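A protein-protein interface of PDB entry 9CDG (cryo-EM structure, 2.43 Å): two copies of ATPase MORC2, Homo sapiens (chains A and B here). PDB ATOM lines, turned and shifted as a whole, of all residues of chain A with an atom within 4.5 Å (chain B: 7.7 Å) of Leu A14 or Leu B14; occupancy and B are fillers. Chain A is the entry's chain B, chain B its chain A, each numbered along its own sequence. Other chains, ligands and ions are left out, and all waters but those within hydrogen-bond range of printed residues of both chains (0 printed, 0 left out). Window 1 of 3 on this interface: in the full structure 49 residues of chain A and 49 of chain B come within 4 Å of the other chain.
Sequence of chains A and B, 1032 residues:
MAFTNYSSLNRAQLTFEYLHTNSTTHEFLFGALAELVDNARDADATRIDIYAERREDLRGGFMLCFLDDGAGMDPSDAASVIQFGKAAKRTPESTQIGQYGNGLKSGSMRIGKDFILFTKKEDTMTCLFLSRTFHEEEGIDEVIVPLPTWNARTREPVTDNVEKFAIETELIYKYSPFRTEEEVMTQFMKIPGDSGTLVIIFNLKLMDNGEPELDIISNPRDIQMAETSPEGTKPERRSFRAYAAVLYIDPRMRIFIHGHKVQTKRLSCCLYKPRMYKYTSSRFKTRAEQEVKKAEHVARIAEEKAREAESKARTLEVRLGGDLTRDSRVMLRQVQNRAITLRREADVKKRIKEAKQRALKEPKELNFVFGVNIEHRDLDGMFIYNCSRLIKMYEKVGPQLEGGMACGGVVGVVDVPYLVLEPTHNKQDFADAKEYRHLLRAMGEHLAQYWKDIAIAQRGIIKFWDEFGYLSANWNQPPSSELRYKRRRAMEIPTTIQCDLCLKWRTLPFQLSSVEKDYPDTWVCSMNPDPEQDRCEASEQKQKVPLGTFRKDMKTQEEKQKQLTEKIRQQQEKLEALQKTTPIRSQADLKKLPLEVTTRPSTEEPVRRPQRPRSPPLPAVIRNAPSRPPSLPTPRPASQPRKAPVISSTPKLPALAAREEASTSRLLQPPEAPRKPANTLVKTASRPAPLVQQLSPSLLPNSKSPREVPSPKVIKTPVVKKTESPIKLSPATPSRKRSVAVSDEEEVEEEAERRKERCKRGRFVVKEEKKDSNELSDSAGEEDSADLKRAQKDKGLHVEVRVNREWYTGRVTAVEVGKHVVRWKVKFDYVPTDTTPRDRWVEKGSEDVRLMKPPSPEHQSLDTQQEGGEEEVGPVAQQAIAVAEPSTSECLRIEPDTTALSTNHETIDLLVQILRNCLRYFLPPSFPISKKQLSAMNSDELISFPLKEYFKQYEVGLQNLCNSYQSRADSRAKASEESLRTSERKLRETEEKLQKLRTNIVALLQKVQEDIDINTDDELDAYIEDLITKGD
NH2 of Arg B11 lies within salt-bridge range of OE2 of Glu A142.
The side-chain hydroxyl of Tyr A18 sits close to the side-chain amide nitrogen of Asn B102 (3.4 Å).
The backbone NH (N) of Gln A13 lies within hydrogen-bond range of the backbone carbonyl oxygen (O) of Ile B82, at 3.4 Å.
The backbone carbonyl oxygen (O) of Gly B85 is in hydrogen-bond range of the side-chain hydroxyl (OG1) of Thr A15 (2.5 Å).
OE1 of Gln B83 sits at hydrogen-bond distance from NE2 of Gln A13.
O of Val B143 lies within hydrogen-bond range of N of Ala A12.
N of Phe A84 lies within hydrogen-bond range of O of Gln B13, at 3.1 Å.
N of Phe B84 is in hydrogen-bond range of O of Gln A13 (3.3 Å).
OH of Tyr A18 is in hydrogen-bond range of OH of Tyr B18, 2.7 Å away.
O of Val A143 is in hydrogen-bond range of N of Ala B12 (2.8 Å).
The backbone NH (N) of Thr A15 lies within hydrogen-bond range of the backbone carbonyl oxygen (O) of Phe B84.
N of Thr B15 sits at hydrogen-bond distance from O of Phe A84.
Among the printed residues, pairs that only touch across the chains: Tyr A18 with Phe B84 (3.2 Å), Phe A84 with Tyr B18 (3.3 Å), Val A143 with Arg B11 (3.3 Å), Leu A14 with Ala B12 (3.3 Å), Ala A12 with Leu B14 (3.3 Å), Gln A83 with Gln B13 (3.4 Å), Leu A14 with Gln B13 (3.4 Å), Gln A83 with Thr B15 (3.4 Å), Ala A12 with Ile B82 (3.4 Å), Tyr A18 with Asn B22 (3.6 Å), Thr A15 with Gln B83 (3.6 Å), Gln A13 with Leu B14 (3.7 Å), Leu A14 with Leu B14 (3.7 Å), Phe A84 with Leu B14 (3.8 Å) and Ala A12 with Phe B84 (3.97 Å).
Hydrophobic or aromatic side chains of chain A that line the printed part of chain B: Ala A12, Leu A14, Tyr A18, Phe A84 and Val A143.
Among the printed residues, Asp or Glu carboxylates within 4 Å of a Lys or Arg side-chain nitrogen of the other chain: Glu A142 with Arg B11.
Leu A14 touches three residues of chain B.
Printed residues of chain B within 4 Å of Tyr A18: Tyr B18 (2.7 Å), Asn B22 (3.6 Å), Phe B84 (3.2 Å) and Asn B102 (3.3 Å).
Of the printed residues of chain B, Gln A83 touches Gln B13 and Thr B15.
Printed residues of chain B within 4 Å of Val A143: Arg B11 (3.3 Å) and Ala B12 (2.8 Å).
Leu B19 touches none of the printed residues of chain A.
Printed residues of chain A within 4 Å of Asn B22: Tyr A18 (3.6 Å).
Ile B144 touches none of the printed residues of chain A.
The nearest residue of chain B that does not touch Leu A14 is Phe B84 (4.2 Å).
The nearest residue of chain A that does not touch Leu B14 is Gln A83 (4.4 Å).
The side-chain amide oxygen of Asn B22 sits close to the side-chain amide oxygen of Asn B102 (2.9 Å).
Ala A12 touches Leu B14, and with the chains exchanged Leu A14 touches Ala B12.
Gln A13 touches Gln B83, and with the chains exchanged Gln A83 touches Gln B13.
Gln A13 touches Phe B84, and with the chains exchanged Phe A84 touches Gln B13.
Tyr A18 touches Phe B84, and with the chains exchanged Phe A84 touches Tyr B18.
10 positions are printed for both chains.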
ATOM      1  N   ALA A  12     -12.392   9.174  35.498  1.00  0.00           N
ATOM      2  CA  ALA A  12     -13.204   9.602  34.366  1.00  0.00           C
ATOM      3  C   ALA A  12     -13.310   8.449  33.381  1.00  0.00           C
ATOM      4  O   ALA A  12     -12.345   8.128  32.680  1.00  0.00           O
ATOM      5  CB  ALA A  12     -12.598  10.834  33.706  1.00  0.00           C
ATOM      6  N   GLN A  13     -14.477   7.818  33.332  1.00  0.00           N
ATOM      7  CA  GLN A  13     -14.689   6.631  32.526  1.00  0.00           C
ATOM      8  C   GLN A  13     -15.254   7.008  31.162  1.00  0.00           C
ATOM      9  O   GLN A  13     -15.412   8.180  30.818  1.00  0.00           O
ATOM     10  CB  GLN A  13     -15.614   5.655  33.249  1.00  0.00           C
ATOM     11  CG  GLN A  13     -15.165   5.312  34.649  1.00  0.00           C
ATOM     12  CD  GLN A  13     -15.700   3.979  35.115  1.00  0.00           C
ATOM     13  OE1 GLN A  13     -14.945   3.026  35.305  1.00  0.00           O
ATOM     14  NE2 GLN A  13     -17.012   3.902  35.302  1.00  0.00           N
ATOM     15  N   LEU A  14     -15.554   5.984  30.373  1.00  0.00           N
ATOM     16  CA  LEU A  14     -16.100   6.142  29.035  1.00  0.00           C
ATOM     17  C   LEU A  14     -17.484   5.521  28.968  1.00  0.00           C
ATOM     18  O   LEU A  14     -17.749   4.500  29.608  1.00  0.00           O
ATOM     19  CB  LEU A  14     -15.199   5.491  27.998  1.00  0.00           C
ATOM     20  CG  LEU A  14     -14.022   6.358  27.592  1.00  0.00           C
ATOM     21  CD1 LEU A  14     -13.033   5.592  26.750  1.00  0.00           C
ATOM     22  CD2 LEU A  14     -14.557   7.527  26.843  1.00  0.00           C
ATOM     23  N   THR A  15     -18.365   6.145  28.197  1.00  0.00           N
ATOM     24  CA  THR A  15     -19.698   5.620  27.963  1.00  0.00           C
ATOM     25  C   THR A  15     -19.894   5.360  26.476  1.00  0.00           C
ATOM     26  O   THR A  15     -19.070   5.749  25.645  1.00  0.00           O
ATOM     27  CB  THR A  15     -20.779   6.574  28.484  1.00  0.00           C
ATOM     28  OG1 THR A  15     -20.730   7.802  27.749  1.00  0.00           O
ATOM     29  CG2 THR A  15     -20.585   6.861  29.963  1.00  0.00           C
ATOM     30  N   TYR A  18     -20.158   8.419  23.983  1.00  0.00           N
ATOM     31  CA  TYR A  18     -18.973   9.204  23.705  1.00  0.00           C
ATOM     32  C   TYR A  18     -18.284   8.749  22.426  1.00  0.00           C
ATOM     33  O   TYR A  18     -17.508   9.516  21.858  1.00  0.00           O
ATOM     34  CB  TYR A  18     -17.988   9.142  24.864  1.00  0.00           C
ATOM     35  CG  TYR A  18     -16.931  10.194  24.724  1.00  0.00           C
ATOM     36  CD1 TYR A  18     -17.276  11.532  24.762  1.00  0.00           C
ATOM     37  CD2 TYR A  18     -15.617   9.864  24.453  1.00  0.00           C
ATOM     38  CE1 TYR A  18     -16.335  12.508  24.604  1.00  0.00           C
ATOM     39  CE2 TYR A  18     -14.665  10.833  24.301  1.00  0.00           C
ATOM     40  CZ  TYR A  18     -15.030  12.159  24.372  1.00  0.00           C
ATOM     41  OH  TYR A  18     -14.096  13.151  24.212  1.00  0.00           O
ATOM     42  N   GLN A  83      -7.132   2.714  25.091  1.00  0.00           N
ATOM     43  CA  GLN A  83      -6.698   3.782  25.978  1.00  0.00           C
ATOM     44  C   GLN A  83      -6.642   5.069  25.171  1.00  0.00           C
ATOM     45  O   GLN A  83      -5.742   5.250  24.345  1.00  0.00           O
ATOM     46  CB  GLN A  83      -5.339   3.451  26.583  1.00  0.00           C
ATOM     47  CG  GLN A  83      -5.322   2.172  27.393  1.00  0.00           C
ATOM     48  CD  GLN A  83      -5.487   2.420  28.876  1.00  0.00           C
ATOM     49  OE1 GLN A  83      -5.860   3.514  29.296  1.00  0.00           O
ATOM     50  NE2 GLN A  83      -5.213   1.400  29.679  1.00  0.00           N
ATOM     51  N   PHE A  84      -7.609   5.955  25.392  1.00  0.00           N
ATOM     52  CA  PHE A  84      -7.728   7.172  24.597  1.00  0.00           C
ATOM     53  C   PHE A  84      -6.613   8.134  24.980  1.00  0.00           C
ATOM     54  O   PHE A  84      -6.522   8.562  26.132  1.00  0.00           O
ATOM     55  CB  PHE A  84      -9.094   7.814  24.814  1.00  0.00           C
ATOM     56  CG  PHE A  84     -10.191   7.229  23.965  1.00  0.00           C
ATOM     57  CD1 PHE A  84     -10.547   5.894  24.079  1.00  0.00           C
ATOM     58  CD2 PHE A  84     -10.882   8.021  23.065  1.00  0.00           C
ATOM     59  CE1 PHE A  84     -11.555   5.359  23.306  1.00  0.00           C
ATOM     60  CE2 PHE A  84     -11.895   7.490  22.290  1.00  0.00           C
ATOM     61  CZ  PHE A  84     -12.231   6.157  22.413  1.00  0.00           C
ATOM     62  N   ASP A 141     -23.562   0.230  28.851  1.00  0.00           N
ATOM     63  CA  ASP A 141     -23.191   1.637  28.762  1.00  0.00           C
ATOM     64  C   ASP A 141     -21.706   1.838  28.507  1.00  0.00           C
ATOM     65  O   ASP A 141     -21.331   2.780  27.803  1.00  0.00           O
ATOM     66  CB  ASP A 141     -23.601   2.372  30.040  1.00  0.00           C
ATOM     67  CG  ASP A 141     -23.353   1.551  31.292  1.00  0.00           C
ATOM     68  OD1 ASP A 141     -23.033   2.147  32.341  1.00  0.00           O
ATOM     69  OD2 ASP A 141     -23.487   0.311  31.234  1.00  0.00           O
ATOM     70  N   GLU A 142     -20.855   0.974  29.054  1.00  0.00           N
ATOM     71  CA  GLU A 142     -19.416   1.132  28.922  1.00  0.00           C
ATOM     72  C   GLU A 142     -18.966   0.788  27.506  1.00  0.00           C
ATOM     73  O   GLU A 142     -19.719   0.246  26.694  1.00  0.00           O
ATOM     74  CB  GLU A 142     -18.683   0.256  29.932  1.00  0.00           C
ATOM     75  CG  GLU A 142     -19.287   0.256  31.313  1.00  0.00           C
ATOM     76  CD  GLU A 142     -18.748  -0.865  32.169  1.00  0.00           C
ATOM     77  OE1 GLU A 142     -17.640  -0.714  32.722  1.00  0.00           O
ATOM     78  OE2 GLU A 142     -19.432  -1.901  32.289  1.00  0.00           O
ATOM     79  N   VAL A 143     -17.714   1.104  27.211  1.00  0.00           N
ATOM     80  CA  VAL A 143     -17.125   0.837  25.904  1.00  0.00           C
ATOM     81  C   VAL A 143     -16.331  -0.456  26.055  1.00  0.00           C
ATOM     82  O   VAL A 143     -15.154  -0.452  26.414  1.00  0.00           O
ATOM     83  CB  VAL A 143     -16.263   1.998  25.427  1.00  0.00           C
ATOM     84  CG1 VAL A 143     -15.947   1.846  23.985  1.00  0.00           C
ATOM     85  CG2 VAL A 143     -16.982   3.283  25.644  1.00  0.00           C
ATOM     86  N   ARG B  11     -11.994  -2.961  28.571  1.00  0.00           N
ATOM     87  CA  ARG B  11     -12.812  -1.776  28.380  1.00  0.00           C
ATOM     88  C   ARG B  11     -11.943  -0.633  27.886  1.00  0.00           C
ATOM     89  O   ARG B  11     -10.758  -0.548  28.217  1.00  0.00           O
ATOM     90  CB  ARG B  11     -13.511  -1.350  29.674  1.00  0.00           C
ATOM     91  CG  ARG B  11     -14.938  -1.818  29.786  1.00  0.00           C
ATOM     92  CD  ARG B  11     -15.025  -3.031  30.673  1.00  0.00           C
ATOM     93  NE  ARG B  11     -16.393  -3.298  31.089  1.00  0.00           N
ATOM     94  CZ  ARG B  11     -16.783  -4.423  31.670  1.00  0.00           C
ATOM     95  NH1 ARG B  11     -15.930  -5.402  31.916  1.00  0.00           N
ATOM     96  NH2 ARG B  11     -18.060  -4.570  32.006  1.00  0.00           N
ATOM     97  N   ALA B  12     -12.542   0.245  27.091  1.00  0.00           N
ATOM     98  CA  ALA B  12     -11.834   1.440  26.661  1.00  0.00           C
ATOM     99  C   ALA B  12     -11.736   2.417  27.819  1.00  0.00           C
ATOM    100  O   ALA B  12     -12.740   2.741  28.460  1.00  0.00           O
ATOM    101  CB  ALA B  12     -12.538   2.088  25.474  1.00  0.00           C
ATOM    102  N   GLN B  13     -10.526   2.885  28.088  1.00  0.00           N
ATOM    103  CA  GLN B  13     -10.248   3.746  29.223  1.00  0.00           C
ATOM    104  C   GLN B  13      -9.878   5.139  28.740  1.00  0.00           C
ATOM    105  O   GLN B  13      -9.755   5.401  27.543  1.00  0.00           O
ATOM    106  CB  GLN B  13      -9.119   3.174  30.084  1.00  0.00           C
ATOM    107  CG  GLN B  13      -9.210   1.685  30.299  1.00  0.00           C
ATOM    108  CD  GLN B  13      -9.656   1.337  31.698  1.00  0.00           C
ATOM    109  OE1 GLN B  13     -10.746   1.713  32.124  1.00  0.00           O
ATOM    110  NE2 GLN B  13      -8.813   0.617  32.426  1.00  0.00           N
ATOM    111  N   LEU B  14      -9.701   6.034  29.701  1.00  0.00           N
ATOM    112  CA  LEU B  14      -9.254   7.389  29.437  1.00  0.00           C
ATOM    113  C   LEU B  14      -7.870   7.587  30.028  1.00  0.00           C
ATOM    114  O   LEU B  14      -7.574   7.096  31.120  1.00  0.00           O
ATOM    115  CB  LEU B  14     -10.215   8.416  30.030  1.00  0.00           C
ATOM    116  CG  LEU B  14     -11.507   8.633  29.259  1.00  0.00           C
ATOM    117  CD1 LEU B  14     -12.255   9.828  29.806  1.00  0.00           C
ATOM    118  CD2 LEU B  14     -11.206   8.805  27.797  1.00  0.00           C
ATOM    119  N   THR B  15      -7.023   8.301  29.301  1.00  0.00           N
ATOM    120  CA  THR B  15      -5.690   8.618  29.778  1.00  0.00           C
ATOM    121  C   THR B  15      -5.566  10.119  29.982  1.00  0.00           C
ATOM    122  O   THR B  15      -6.460  10.892  29.626  1.00  0.00           O
ATOM    123  CB  THR B  15      -4.610   8.122  28.809  1.00  0.00           C
ATOM    124  OG1 THR B  15      -4.713   8.836  27.574  1.00  0.00           O
ATOM    125  CG2 THR B  15      -4.773   6.639  28.544  1.00  0.00           C
ATOM    126  N   PHE B  16      -4.424  10.497  30.565  1.00  0.00           N
ATOM    127  CA  PHE B  16      -4.121  11.886  30.904  1.00  0.00           C
ATOM    128  C   PHE B  16      -4.170  12.773  29.659  1.00  0.00           C
ATOM    129  O   PHE B  16      -4.837  13.815  29.655  1.00  0.00           O
ATOM    130  CB  PHE B  16      -2.733  11.918  31.564  1.00  0.00           C
ATOM    131  CG  PHE B  16      -2.268  13.272  32.086  1.00  0.00           C
ATOM    132  CD1 PHE B  16      -3.113  14.368  32.235  1.00  0.00           C
ATOM    133  CD2 PHE B  16      -0.926  13.443  32.378  1.00  0.00           C
ATOM    134  CE1 PHE B  16      -2.641  15.569  32.669  1.00  0.00           C
ATOM    135  CE2 PHE B  16      -0.449  14.653  32.826  1.00  0.00           C
ATOM    136  CZ  PHE B  16      -1.313  15.716  32.969  1.00  0.00           C
ATOM    137  N   GLU B  17      -3.499  12.362  28.585  1.00  0.00           N
ATOM    138  CA  GLU B  17      -3.375  13.215  27.410  1.00  0.00           C
ATOM    139  C   GLU B  17      -4.675  13.353  26.633  1.00  0.00           C
ATOM    140  O   GLU B  17      -4.769  14.225  25.759  1.00  0.00           O
ATOM    141  CB  GLU B  17      -2.273  12.677  26.499  1.00  0.00           C
ATOM    142  CG  GLU B  17      -1.102  12.070  27.255  1.00  0.00           C
ATOM    143  CD  GLU B  17       0.022  13.059  27.513  1.00  0.00           C
ATOM    144  OE1 GLU B  17      -0.248  14.275  27.593  1.00  0.00           O
ATOM    145  OE2 GLU B  17       1.181  12.615  27.641  1.00  0.00           O
ATOM    146  N   TYR B  18      -5.688  12.544  26.943  1.00  0.00           N
ATOM    147  CA  TYR B  18      -6.966  12.717  26.279  1.00  0.00           C
ATOM    148  C   TYR B  18      -7.683  13.978  26.739  1.00  0.00           C
ATOM    149  O   TYR B  18      -8.537  14.480  26.011  1.00  0.00           O
ATOM    150  CB  TYR B  18      -7.882  11.521  26.506  1.00  0.00           C
ATOM    151  CG  TYR B  18      -9.035  11.565  25.548  1.00  0.00           C
ATOM    152  CD1 TYR B  18      -8.800  11.631  24.189  1.00  0.00           C
ATOM    153  CD2 TYR B  18     -10.337  11.694  25.993  1.00  0.00           C
ATOM    154  CE1 TYR B  18      -9.829  11.720  23.301  1.00  0.00           C
ATOM    155  CE2 TYR B  18     -11.381  11.777  25.104  1.00  0.00           C
ATOM    156  CZ  TYR B  18     -11.114  11.794  23.751  1.00  0.00           C
ATOM    157  OH  TYR B  18     -12.117  11.889  22.821  1.00  0.00           O
ATOM    158  N   LEU B  19      -7.354  14.507  27.920  1.00  0.00           N
ATOM    159  CA  LEU B  19      -7.901  15.799  28.319  1.00  0.00           C
ATOM    160  C   LEU B  19      -7.416  16.905  27.392  1.00  0.00           C
ATOM    161  O   LEU B  19      -8.201  17.757  26.967  1.00  0.00           O
ATOM    162  CB  LEU B  19      -7.521  16.103  29.766  1.00  0.00           C
ATOM    163  CG  LEU B  19      -8.092  15.151  30.816  1.00  0.00           C
ATOM    164  CD1 LEU B  19      -7.630  15.556  32.197  1.00  0.00           C
ATOM    165  CD2 LEU B  19      -9.605  15.121  30.746  1.00  0.00           C
ATOM    166  N   ASN B  22      -9.137  16.248  23.955  1.00  0.00           N
ATOM    167  CA  ASN B  22     -10.483  16.791  24.062  1.00  0.00           C
ATOM    168  C   ASN B  22     -10.475  18.312  24.043  1.00  0.00           C
ATOM    169  O   ASN B  22     -11.387  18.940  23.495  1.00  0.00           O
ATOM    170  CB  ASN B  22     -11.105  16.271  25.356  1.00  0.00           C
ATOM    171  CG  ASN B  22     -12.585  16.477  25.420  1.00  0.00           C
ATOM    172  OD1 ASN B  22     -13.254  16.612  24.402  1.00  0.00           O
ATOM    173  ND2 ASN B  22     -13.112  16.518  26.634  1.00  0.00           N
ATOM    174  N   ILE B  82     -18.076  13.205  35.002  1.00  0.00           N
ATOM    175  CA  ILE B  82     -16.853  12.616  34.459  1.00  0.00           C
ATOM    176  C   ILE B  82     -17.113  11.350  33.661  1.00  0.00           C
ATOM    177  O   ILE B  82     -16.173  10.796  33.082  1.00  0.00           O
ATOM    178  CB  ILE B  82     -15.835  12.321  35.573  1.00  0.00           C
ATOM    179  CG1 ILE B  82     -16.363  11.239  36.513  1.00  0.00           C
ATOM    180  CG2 ILE B  82     -15.531  13.584  36.340  1.00  0.00           C
ATOM    181  CD1 ILE B  82     -15.406  10.873  37.618  1.00  0.00           C
ATOM    182  N   GLN B  83     -18.350  10.867  33.628  1.00  0.00           N
ATOM    183  CA  GLN B  83     -18.748   9.862  32.648  1.00  0.00           C
ATOM    184  C   GLN B  83     -18.881  10.565  31.309  1.00  0.00           C
ATOM    185  O   GLN B  83     -19.840  11.302  31.075  1.00  0.00           O
ATOM    186  CB  GLN B  83     -20.053   9.194  33.057  1.00  0.00           C
ATOM    187  CG  GLN B  83     -19.977   8.441  34.367  1.00  0.00           C
ATOM    188  CD  GLN B  83     -19.084   7.224  34.282  1.00  0.00           C
ATOM    189  OE1 GLN B  83     -18.138   7.080  35.053  1.00  0.00           O
ATOM    190  NE2 GLN B  83     -19.380   6.340  33.339  1.00  0.00           N
ATOM    191  N   PHE B  84     -17.903  10.355  30.431  1.00  0.00           N
ATOM    192  CA  PHE B  84     -17.850  11.063  29.159  1.00  0.00           C
ATOM    193  C   PHE B  84     -18.956  10.548  28.248  1.00  0.00           C
ATOM    194  O   PHE B  84     -19.001   9.357  27.931  1.00  0.00           O
ATOM    195  CB  PHE B  84     -16.485  10.870  28.505  1.00  0.00           C
ATOM    196  CG  PHE B  84     -15.444  11.857  28.954  1.00  0.00           C
ATOM    197  CD1 PHE B  84     -15.133  12.004  30.297  1.00  0.00           C
ATOM    198  CD2 PHE B  84     -14.765  12.632  28.030  1.00  0.00           C
ATOM    199  CE1 PHE B  84     -14.173  12.904  30.708  1.00  0.00           C
ATOM    200  CE2 PHE B  84     -13.801  13.535  28.436  1.00  0.00           C
ATOM    201  CZ  PHE B  84     -13.507  13.669  29.777  1.00  0.00           C
ATOM    202  N   GLY B  85     -19.875  11.430  27.877  1.00  0.00           N
ATOM    203  CA  GLY B  85     -21.014  11.044  27.071  1.00  0.00           C
ATOM    204  C   GLY B  85     -22.183  10.676  27.958  1.00  0.00           C
ATOM    205  O   GLY B  85     -22.170   9.610  28.576  1.00  0.00           O
ATOM    206  N   ASN B 102     -19.853  16.003  26.958  1.00  0.00           N
ATOM    207  CA  ASN B 102     -18.429  16.221  26.759  1.00  0.00           C
ATOM    208  C   ASN B 102     -18.002  17.661  26.993  1.00  0.00           C
ATOM    209  O   ASN B 102     -16.852  17.921  27.367  1.00  0.00           O
ATOM    210  CB  ASN B 102     -18.056  15.812  25.339  1.00  0.00           C
ATOM    211  CG  ASN B 102     -16.581  15.873  25.093  1.00  0.00           C
ATOM    212  OD1 ASN B 102     -16.134  16.358  24.061  1.00  0.00           O
ATOM    213  ND2 ASN B 102     -15.810  15.379  26.044  1.00  0.00           N
ATOM    214  N   LYS B 105     -15.944  19.248  29.901  1.00  0.00           N
ATOM    215  CA  LYS B 105     -14.601  18.688  29.976  1.00  0.00           C
ATOM    216  C   LYS B 105     -13.730  19.174  28.828  1.00  0.00           C
ATOM    217  O   LYS B 105     -12.521  19.361  28.996  1.00  0.00           O
ATOM    218  CB  LYS B 105     -14.677  17.163  29.987  1.00  0.00           C
ATOM    219  CG  LYS B 105     -15.045  16.569  31.333  1.00  0.00           C
ATOM    220  CD  LYS B 105     -16.544  16.343  31.464  1.00  0.00           C
ATOM    221  CE  LYS B 105     -17.076  15.448  30.364  1.00  0.00           C
ATOM    222  NZ  LYS B 105     -18.522  15.167  30.548  1.00  0.00           N
ATOM    223  N   ASP B 141      -1.273   8.226  34.921  1.00  0.00           N
ATOM    224  CA  ASP B 141      -1.665   7.929  33.548  1.00  0.00           C
ATOM    225  C   ASP B 141      -3.166   8.090  33.356  1.00  0.00           C
ATOM    226  O   ASP B 141      -3.611   8.608  32.327  1.00  0.00           O
ATOM    227  CB  ASP B 141      -1.227   6.515  33.174  1.00  0.00           C
ATOM    228  CG  ASP B 141      -1.427   5.523  34.305  1.00  0.00           C
ATOM    229  OD1 ASP B 141      -1.778   4.358  34.020  1.00  0.00           O
ATOM    230  OD2 ASP B 141      -1.235   5.905  35.479  1.00  0.00           O
ATOM    231  N   GLU B 142      -3.957   7.673  34.340  1.00  0.00           N
ATOM    232  CA  GLU B 142      -5.408   7.700  34.231  1.00  0.00           C
ATOM    233  C   GLU B 142      -5.924   9.116  34.471  1.00  0.00           C
ATOM    234  O   GLU B 142      -5.161  10.064  34.662  1.00  0.00           O
ATOM    235  CB  GLU B 142      -6.030   6.718  35.217  1.00  0.00           C
ATOM    236  CG  GLU B 142      -5.377   5.358  35.235  1.00  0.00           C
ATOM    237  CD  GLU B 142      -5.756   4.559  36.461  1.00  0.00           C
ATOM    238  OE1 GLU B 142      -6.852   3.962  36.467  1.00  0.00           O
ATOM    239  OE2 GLU B 142      -4.961   4.532  37.421  1.00  0.00           O
ATOM    240  N   VAL B 143      -7.239   9.268  34.470  1.00  0.00           N
ATOM    241  CA  VAL B 143      -7.889  10.547  34.736  1.00  0.00           C
ATOM    242  C   VAL B 143      -8.611  10.389  36.068  1.00  0.00           C
ATOM    243  O   VAL B 143      -9.775   9.989  36.119  1.00  0.00           O
ATOM    244  CB  VAL B 143      -8.856  10.950  33.624  1.00  0.00           C
ATOM    245  CG1 VAL B 143      -9.136  12.414  33.687  1.00  0.00           C
ATOM    246  CG2 VAL B 143      -8.284  10.603  32.290  1.00  0.00           C
ATOM    247  N   ILE B 144      -7.926  10.721  37.155  1.00  0.00           N
ATOM    248  CA  ILE B 144      -8.445  10.547  38.504  1.00  0.00           C
ATOM    249  C   ILE B 144      -9.088  11.848  38.954  1.00  0.00           C
ATOM    250  O   ILE B 144      -8.439  12.901  38.965  1.00  0.00           O
ATOM    251  CB  ILE B 144      -7.334  10.113  39.472  1.00  0.00           C
ATOM    252  CG1 ILE B 144      -6.810   8.734  39.080  1.00  0.00           C
ATOM    253  CG2 ILE B 144      -7.845  10.108  40.891  1.00  0.00           C
ATOM    254  CD1 ILE B 144      -5.736   8.211  39.991  1.00  0.00           C
